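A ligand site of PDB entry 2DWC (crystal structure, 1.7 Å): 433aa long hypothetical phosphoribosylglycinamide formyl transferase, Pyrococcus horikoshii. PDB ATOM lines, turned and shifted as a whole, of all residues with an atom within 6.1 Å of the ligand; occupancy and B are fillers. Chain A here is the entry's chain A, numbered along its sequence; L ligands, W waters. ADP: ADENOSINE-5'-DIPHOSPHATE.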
ATOM      1  N   ARG A 121       2.411  14.094  21.221  1.00  0.00           N
ATOM      2  CA  ARG A 121       1.889  14.064  19.860  1.00  0.00           C
ATOM      3  C   ARG A 121       0.514  13.426  19.684  1.00  0.00           C
ATOM      4  O   ARG A 121      -0.286  13.905  18.883  1.00  0.00           O
ATOM      5  CB  ARG A 121       2.865  13.363  18.919  1.00  0.00           C
ATOM      6  CG  ARG A 121       4.106  14.141  18.580  1.00  0.00           C
ATOM      7  CD  ARG A 121       4.814  13.426  17.483  1.00  0.00           C
ATOM      8  NE  ARG A 121       6.207  13.808  17.354  1.00  0.00           N
ATOM      9  CZ  ARG A 121       6.626  14.936  16.809  1.00  0.00           C
ATOM     10  NH1 ARG A 121       5.741  15.813  16.330  1.00  0.00           N
ATOM     11  NH2 ARG A 121       7.925  15.182  16.687  1.00  0.00           N
ATOM     12  N   SER A 137      -3.294  15.805   8.287  1.00  0.00           N
ATOM     13  CA  SER A 137      -2.797  14.750   7.409  1.00  0.00           C
ATOM     14  C   SER A 137      -3.483  13.477   7.891  1.00  0.00           C
ATOM     15  O   SER A 137      -3.827  13.351   9.072  1.00  0.00           O
ATOM     16  CB  SER A 137      -1.278  14.612   7.600  1.00  0.00           C
ATOM     17  OG  SER A 137      -0.952  14.301   8.961  1.00  0.00           O
ATOM     18  N   HIS A 160       5.495   9.828   6.983  1.00  0.00           N
ATOM     19  CA  HIS A 160       6.285  10.331   8.094  1.00  0.00           C
ATOM     20  C   HIS A 160       5.947   9.561   9.346  1.00  0.00           C
ATOM     21  O   HIS A 160       4.779   9.401   9.671  1.00  0.00           O
ATOM     22  CB  HIS A 160       5.993  11.831   8.320  1.00  0.00           C
ATOM     23  CG  HIS A 160       6.277  12.691   7.120  1.00  0.00           C
ATOM     24  ND1 HIS A 160       7.467  13.365   6.960  1.00  0.00           N
ATOM     25  CD2 HIS A 160       5.553  12.927   6.001  1.00  0.00           C
ATOM     26  CE1 HIS A 160       7.473  13.982   5.789  1.00  0.00           C
ATOM     27  NE2 HIS A 160       6.325  13.733   5.187  1.00  0.00           N
ATOM     28  N   LYS A 162       6.659   9.449  13.481  1.00  0.00           N
ATOM     29  CA  LYS A 162       7.120  10.316  14.574  1.00  0.00           C
ATOM     30  C   LYS A 162       6.854   9.681  15.931  1.00  0.00           C
ATOM     31  O   LYS A 162       5.790   9.119  16.164  1.00  0.00           O
ATOM     32  CB  LYS A 162       6.411  11.673  14.520  1.00  0.00           C
ATOM     33  CG  LYS A 162       6.328  12.291  13.127  1.00  0.00           C
ATOM     34  CD  LYS A 162       5.446  13.558  13.105  1.00  0.00           C
ATOM     35  CE  LYS A 162       5.222  14.038  11.658  1.00  0.00           C
ATOM     36  NZ  LYS A 162       4.404  15.274  11.556  1.00  0.00           N
ATOM     37  N   MET A 165       6.614  10.784  21.970  1.00  0.00           N
ATOM     38  CA  MET A 165       7.374  11.474  23.014  1.00  0.00           C
ATOM     39  C   MET A 165       6.512  11.745  24.251  1.00  0.00           C
ATOM     40  O   MET A 165       5.655  10.933  24.623  1.00  0.00           O
ATOM     41  CB  MET A 165       7.940  12.794  22.483  1.00  0.00           C
ATOM     42  CG  MET A 165       8.802  12.659  21.241  1.00  0.00           C
ATOM     43  SD  MET A 165       9.015  14.228  20.332  1.00  0.00           S
ATOM     44  CE  MET A 165      10.781  14.586  20.630  1.00  0.00           C
ATOM     45  N   SER A 172      11.804  10.713  14.635  1.00  0.00           N
ATOM     46  CA  SER A 172      11.123  10.922  13.355  1.00  0.00           C
ATOM     47  C   SER A 172      11.902  10.378  12.170  1.00  0.00           C
ATOM     48  O   SER A 172      13.129  10.397  12.154  1.00  0.00           O
ATOM     49  CB  SER A 172      10.869  12.415  13.094  1.00  0.00           C
ATOM     50  OG  SER A 172       9.905  12.929  14.000  1.00  0.00           O
ATOM     51  N   GLU A 202       2.093   9.373   9.458  1.00  0.00           N
ATOM     52  CA  GLU A 202       1.315  10.322   8.690  1.00  0.00           C
ATOM     53  C   GLU A 202       1.576  10.327   7.205  1.00  0.00           C
ATOM     54  O   GLU A 202       2.720  10.152   6.747  1.00  0.00           O
ATOM     55  CB  GLU A 202       1.605  11.738   9.181  1.00  0.00           C
ATOM     56  CG  GLU A 202       1.456  11.987  10.643  1.00  0.00           C
ATOM     57  CD  GLU A 202       1.819  13.444  10.986  1.00  0.00           C
ATOM     58  OE1 GLU A 202       1.803  14.301  10.063  1.00  0.00           O
ATOM     59  OE2 GLU A 202       2.111  13.718  12.159  1.00  0.00           O
ATOM     60  N   GLU A 203       0.500  10.590   6.484  1.00  0.00           N
ATOM     61  CA  GLU A 203       0.494  10.743   5.041  1.00  0.00           C
ATOM     62  C   GLU A 203       1.333  11.964   4.696  1.00  0.00           C
ATOM     63  O   GLU A 203       1.258  13.002   5.364  1.00  0.00           O
ATOM     64  CB  GLU A 203      -0.945  10.957   4.581  1.00  0.00           C
ATOM     65  CG  GLU A 203      -1.106  11.804   3.340  1.00  0.00           C
ATOM     66  CD  GLU A 203      -2.533  12.313   3.155  1.00  0.00           C
ATOM     67  OE1 GLU A 203      -3.166  12.801   4.133  1.00  0.00           O
ATOM     68  OE2 GLU A 203      -3.017  12.252   2.012  1.00  0.00           O
ATOM     69  N   HIS A 204       2.127  11.862   3.635  1.00  0.00           N
ATOM     70  CA  HIS A 204       2.941  12.972   3.210  1.00  0.00           C
ATOM     71  C   HIS A 204       2.127  14.013   2.447  1.00  0.00           C
ATOM     72  O   HIS A 204       1.489  13.685   1.442  1.00  0.00           O
ATOM     73  CB  HIS A 204       4.065  12.491   2.291  1.00  0.00           C
ATOM     74  CG  HIS A 204       4.911  13.602   1.750  1.00  0.00           C
ATOM     75  ND1 HIS A 204       5.780  14.320   2.545  1.00  0.00           N
ATOM     76  CD2 HIS A 204       4.976  14.163   0.514  1.00  0.00           C
ATOM     77  CE1 HIS A 204       6.340  15.278   1.824  1.00  0.00           C
ATOM     78  NE2 HIS A 204       5.864  15.202   0.588  1.00  0.00           N
ATOM     79  N   ILE A 205       2.164  15.261   2.917  1.00  0.00           N
ATOM     80  CA  ILE A 205       1.451  16.340   2.234  1.00  0.00           C
ATOM     81  C   ILE A 205       2.456  17.080   1.346  1.00  0.00           C
ATOM     82  O   ILE A 205       3.475  17.592   1.834  1.00  0.00           O
ATOM     83  CB  ILE A 205       0.847  17.349   3.246  1.00  0.00           C
ATOM     84  CG1 ILE A 205      -0.123  16.642   4.198  1.00  0.00           C
ATOM     85  CG2 ILE A 205       0.136  18.486   2.504  1.00  0.00           C
ATOM     86  CD1 ILE A 205      -1.322  15.974   3.500  1.00  0.00           C
ATOM     87  N   ASP A 206       2.215  17.104   0.041  1.00  0.00           N
ATOM     88  CA  ASP A 206       3.140  17.803  -0.847  1.00  0.00           C
ATOM     89  C   ASP A 206       2.707  19.267  -0.926  1.00  0.00           C
ATOM     90  O   ASP A 206       2.156  19.729  -1.931  1.00  0.00           O
ATOM     91  CB  ASP A 206       3.115  17.160  -2.234  1.00  0.00           C
ATOM     92  CG  ASP A 206       3.977  17.902  -3.232  1.00  0.00           C
ATOM     93  OD1 ASP A 206       5.121  18.268  -2.854  1.00  0.00           O
ATOM     94  OD2 ASP A 206       3.517  18.122  -4.376  1.00  0.00           O
ATOM     95  N   PHE A 207       2.966  19.995   0.151  1.00  0.00           N
ATOM     96  CA  PHE A 207       2.549  21.393   0.231  1.00  0.00           C
ATOM     97  C   PHE A 207       3.404  22.392  -0.538  1.00  0.00           C
ATOM     98  O   PHE A 207       4.544  22.119  -0.874  1.00  0.00           O
ATOM     99  CB  PHE A 207       2.477  21.813   1.711  1.00  0.00           C
ATOM    100  CG  PHE A 207       3.758  21.578   2.469  1.00  0.00           C
ATOM    101  CD1 PHE A 207       3.867  20.515   3.381  1.00  0.00           C
ATOM    102  CD2 PHE A 207       4.864  22.394   2.255  1.00  0.00           C
ATOM    103  CE1 PHE A 207       5.064  20.284   4.056  1.00  0.00           C
ATOM    104  CE2 PHE A 207       6.061  22.173   2.933  1.00  0.00           C
ATOM    105  CZ  PHE A 207       6.176  21.123   3.836  1.00  0.00           C
ATOM    106  N   GLU A 210       4.902  25.794   4.223  1.00  0.00           N
ATOM    107  CA  GLU A 210       4.515  25.509   5.597  1.00  0.00           C
ATOM    108  C   GLU A 210       4.359  26.900   6.196  1.00  0.00           C
ATOM    109  O   GLU A 210       5.154  27.780   5.883  1.00  0.00           O
ATOM    110  CB  GLU A 210       5.674  24.873   6.349  1.00  0.00           C
ATOM    111  CG  GLU A 210       5.715  23.412   6.399  1.00  0.00           C
ATOM    112  CD  GLU A 210       6.932  22.954   7.175  1.00  0.00           C
ATOM    113  OE1 GLU A 210       8.026  22.819   6.580  1.00  0.00           O
ATOM    114  OE2 GLU A 210       6.767  22.744   8.390  1.00  0.00           O
ATOM    115  N   GLN A 237      12.375  24.144   6.649  1.00  0.00           N
ATOM    116  CA  GLN A 237      13.361  23.573   7.543  1.00  0.00           C
ATOM    117  C   GLN A 237      14.020  22.306   7.033  1.00  0.00           C
ATOM    118  O   GLN A 237      13.472  21.594   6.204  1.00  0.00           O
ATOM    119  CB  GLN A 237      12.740  23.307   8.902  1.00  0.00           C
ATOM    120  CG  GLN A 237      11.329  22.769   8.884  1.00  0.00           C
ATOM    121  CD  GLN A 237      10.834  22.548  10.296  1.00  0.00           C
ATOM    122  OE1 GLN A 237      11.076  21.500  10.895  1.00  0.00           O
ATOM    123  NE2 GLN A 237      10.159  23.556  10.843  1.00  0.00           N
ATOM    124  N   ILE A 238      15.211  22.054   7.564  1.00  0.00           N
ATOM    125  CA  ILE A 238      15.978  20.866   7.209  1.00  0.00           C
ATOM    126  C   ILE A 238      15.613  19.775   8.203  1.00  0.00           C
ATOM    127  O   ILE A 238      16.474  19.181   8.856  1.00  0.00           O
ATOM    128  CB  ILE A 238      17.495  21.134   7.291  1.00  0.00           C
ATOM    129  CG1 ILE A 238      17.812  22.537   6.736  1.00  0.00           C
ATOM    130  CG2 ILE A 238      18.247  20.037   6.546  1.00  0.00           C
ATOM    131  CD1 ILE A 238      17.217  22.832   5.371  1.00  0.00           C
ATOM    132  N   ASP A 239      14.310  19.532   8.315  1.00  0.00           N
ATOM    133  CA  ASP A 239      13.781  18.512   9.213  1.00  0.00           C
ATOM    134  C   ASP A 239      14.238  18.720  10.645  1.00  0.00           C
ATOM    135  O   ASP A 239      15.401  18.460  10.987  1.00  0.00           O
ATOM    136  CB  ASP A 239      14.182  17.119   8.718  1.00  0.00           C
ATOM    137  CG  ASP A 239      13.657  16.809   7.320  1.00  0.00           C
ATOM    138  OD1 ASP A 239      12.411  16.773   7.142  1.00  0.00           O
ATOM    139  OD2 ASP A 239      14.483  16.615   6.395  1.00  0.00           O
ATOM    140  N   GLY A 240      13.321  19.190  11.481  1.00  0.00           N
ATOM    141  CA  GLY A 240      13.631  19.421  12.874  1.00  0.00           C
ATOM    142  C   GLY A 240      14.052  20.844  13.190  1.00  0.00           C
ATOM    143  O   GLY A 240      13.707  21.377  14.250  1.00  0.00           O
ATOM    144  N   GLU A 279       0.973  25.655  13.430  1.00  0.00           N
ATOM    145  CA  GLU A 279       1.671  25.177  12.232  1.00  0.00           C
ATOM    146  C   GLU A 279       0.718  24.505  11.248  1.00  0.00           C
ATOM    147  O   GLU A 279      -0.034  23.631  11.648  1.00  0.00           O
ATOM    148  CB  GLU A 279       2.737  24.158  12.618  1.00  0.00           C
ATOM    149  CG  GLU A 279       3.851  24.767  13.452  1.00  0.00           C
ATOM    150  CD  GLU A 279       4.575  25.833  12.674  1.00  0.00           C
ATOM    151  OE1 GLU A 279       5.040  26.815  13.292  1.00  0.00           O
ATOM    152  OE2 GLU A 279       4.678  25.711  11.423  1.00  0.00           O
ATOM    153  N   PHE A 281       0.112  23.317   6.813  1.00  0.00           N
ATOM    154  CA  PHE A 281       0.664  23.051   5.502  1.00  0.00           C
ATOM    155  C   PHE A 281      -0.357  23.677   4.526  1.00  0.00           C
ATOM    156  O   PHE A 281      -1.568  23.590   4.744  1.00  0.00           O
ATOM    157  CB  PHE A 281       0.739  21.534   5.235  1.00  0.00           C
ATOM    158  CG  PHE A 281       1.584  20.782   6.225  1.00  0.00           C
ATOM    159  CD1 PHE A 281       2.829  21.275   6.622  1.00  0.00           C
ATOM    160  CD2 PHE A 281       1.188  19.536   6.708  1.00  0.00           C
ATOM    161  CE1 PHE A 281       3.640  20.529   7.483  1.00  0.00           C
ATOM    162  CE2 PHE A 281       1.996  18.792   7.559  1.00  0.00           C
ATOM    163  CZ  PHE A 281       3.219  19.287   7.952  1.00  0.00           C
ATOM    164  N   ASN A 290      -1.023  21.049  11.338  1.00  0.00           N
ATOM    165  CA  ASN A 290       0.051  20.102  11.614  1.00  0.00           C
ATOM    166  C   ASN A 290       0.238  19.999  13.127  1.00  0.00           C
ATOM    167  O   ASN A 290       0.063  18.940  13.710  1.00  0.00           O
ATOM    168  CB  ASN A 290       1.327  20.569  10.905  1.00  0.00           C
ATOM    169  CG  ASN A 290       2.563  19.806  11.329  1.00  0.00           C
ATOM    170  OD1 ASN A 290       2.490  18.625  11.643  1.00  0.00           O
ATOM    171  ND2 ASN A 290       3.711  20.499  11.326  1.00  0.00           N
ATOM    172  N   GLU A 291       0.583  21.104  13.793  1.00  0.00           N
ATOM    173  CA  GLU A 291       0.730  21.031  15.241  1.00  0.00           C
ATOM    174  C   GLU A 291       0.657  22.470  15.776  1.00  0.00           C
ATOM    175  O   GLU A 291       0.330  23.358  15.015  1.00  0.00           O
ATOM    176  CB  GLU A 291       2.072  20.413  15.590  1.00  0.00           C
ATOM    177  CG  GLU A 291       3.205  21.124  14.906  1.00  0.00           C
ATOM    178  CD  GLU A 291       4.539  20.457  15.212  1.00  0.00           C
ATOM    179  OE1 GLU A 291       4.513  19.448  15.940  1.00  0.00           O
ATOM    180  OE2 GLU A 291       5.585  20.933  14.732  1.00  0.00           O
HETATM  181  PB  ADP L   1       8.505  18.294  15.055  1.00  0.00           P
HETATM  182  O1B ADP L   1       7.433  18.048  16.040  1.00  0.00           O
HETATM  183  O2B ADP L   1       9.534  19.529  15.200  1.00  0.00           O
HETATM  184  O3B ADP L   1       9.082  17.134  14.103  1.00  0.00           O
HETATM  185  PA  ADP L   1       6.938  18.151  12.725  1.00  0.00           P
HETATM  186  O1A ADP L   1       6.441  16.834  13.205  1.00  0.00           O
HETATM  187  O2A ADP L   1       5.742  19.083  12.178  1.00  0.00           O
HETATM  188  O3A ADP L   1       7.639  19.002  13.897  1.00  0.00           O
HETATM  189  O5' ADP L   1       8.003  18.066  11.517  1.00  0.00           O
HETATM  190  C5' ADP L   1       7.995  19.122  10.553  1.00  0.00           C
HETATM  191  C4' ADP L   1       9.012  18.876   9.441  1.00  0.00           C
HETATM  192  O4' ADP L   1       8.683  17.648   8.767  1.00  0.00           O
HETATM  193  C3' ADP L   1       8.760  19.963   8.382  1.00  0.00           C
HETATM  194  O3' ADP L   1       9.709  19.849   7.316  1.00  0.00           O
HETATM  195  C2' ADP L   1       7.406  19.458   7.882  1.00  0.00           C
HETATM  196  O2' ADP L   1       7.166  20.018   6.592  1.00  0.00           O
HETATM  197  C1' ADP L   1       7.739  17.967   7.734  1.00  0.00           C
HETATM  198  N9  ADP L   1       6.508  17.155   7.866  1.00  0.00           N
HETATM  199  C8  ADP L   1       6.031  16.648   9.006  1.00  0.00           C
HETATM  200  N7  ADP L   1       4.888  15.995   8.761  1.00  0.00           N
HETATM  201  C5  ADP L   1       4.643  16.101   7.458  1.00  0.00           C
HETATM  202  C6  ADP L   1       3.624  15.635   6.628  1.00  0.00           C
HETATM  203  N6  ADP L   1       2.606  14.955   7.126  1.00  0.00           N
HETATM  204  N1  ADP L   1       3.688  15.905   5.318  1.00  0.00           N
HETATM  205  C2  ADP L   1       4.691  16.609   4.809  1.00  0.00           C
HETATM  206  N3  ADP L   1       5.660  17.076   5.568  1.00  0.00           N
HETATM  207  C4  ADP L   1       5.669  16.834   6.886  1.00  0.00           C
HETATM  208  O   HOH W   1       3.187  17.154  13.986  1.00  0.00           O
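The backbone NH (N) of Glu 202 is in hydrogen-bond range of the backbone carbonyl oxygen (O) of His 160 (2.7 Å). NZ of Lys 162 is in salt-bridge range of OE2 of Glu 202, at 2.8 Å. N of Asn 290 lies within hydrogen-bond range of O of Glu 279, at 2.8 Å. The backbone NH (N) of Glu 279 lies within hydrogen-bond range of the backbone carbonyl oxygen (O) of Glu 291 (2.9 Å). The side-chain carboxylate (OE1) of Glu 291 lies within salt-bridge range of the guanidinium group (NH1) of Arg 121. OE1 of Gln 237 lies within hydrogen-bond range of N of Gly 240 (3.3 Å). The side-chain hydroxyl (OG) of Ser 137 sits at hydrogen-bond distance from the side-chain carboxylate (OE1) of Glu 202 (3.0 Å). NE2 of His 160 lies within hydrogen-bond range of ND1 of His 204, at 2.8 Å.
The side-chain carboxylate (OE2) of Glu 291 lies close to an oxygen (O3A) of the ligand, 2.9 Å away. CB of Ser 137 touches N6 of the ligand, at 3.9 Å. ND1 of His 204 touches C2 of the ligand (3.4 Å). Phe 207 touches the ligand. OE1 of Gln 237 touches C4' of the ligand, 3.6 Å away. CZ of Phe 281 touches C5 of the ligand, at 3.5 Å. Hydrophobic or aromatic side chains that line the ligand: His 160, His 204, Ile 205, Phe 207 and Phe 281. Of the 21 residues printed, 14 come within 4 Å of the ligand. The nearest printed residue that does not touch the ligand is Asp 239 (4.1 Å).
The guanidinium group (NH1) of Arg 121 is in salt-bridge range of an oxygen (O1B) of the ligand, 2.8 Å away. The side-chain carboxylate of Glu 210 lies within hydrogen-bond range of an oxygen (O2') of the ligand. OE1 of Glu 202 sits at hydrogen-bond distance from N6 of the ligand. A nitrogen (N6) of the ligand lies within hydrogen-bond range of the backbone carbonyl oxygen (O) of Glu 203, at 3.0 Å. N of Ile 205 lies within hydrogen-bond range of N1 of the ligand (2.9 Å). ND2 of Asn 290 sits at hydrogen-bond distance from O2A of the ligand, 2.6 Å away. The side-chain amino group (NZ) of Lys 162 is in salt-bridge range of an oxygen (O1A) of the ligand (3.0 Å). N1 of the ligand lies close to NE2 of His 160.
Water W1 lies within hydrogen-bond range of the side-chain amide oxygen of Asn 290 (2.9 Å), the side-chain carboxylate of Glu 291 (3.3 Å), the side-chain amino group of Lys 162 (3.3 Å) and an oxygen (O1A) of the ligand (3.4 Å).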
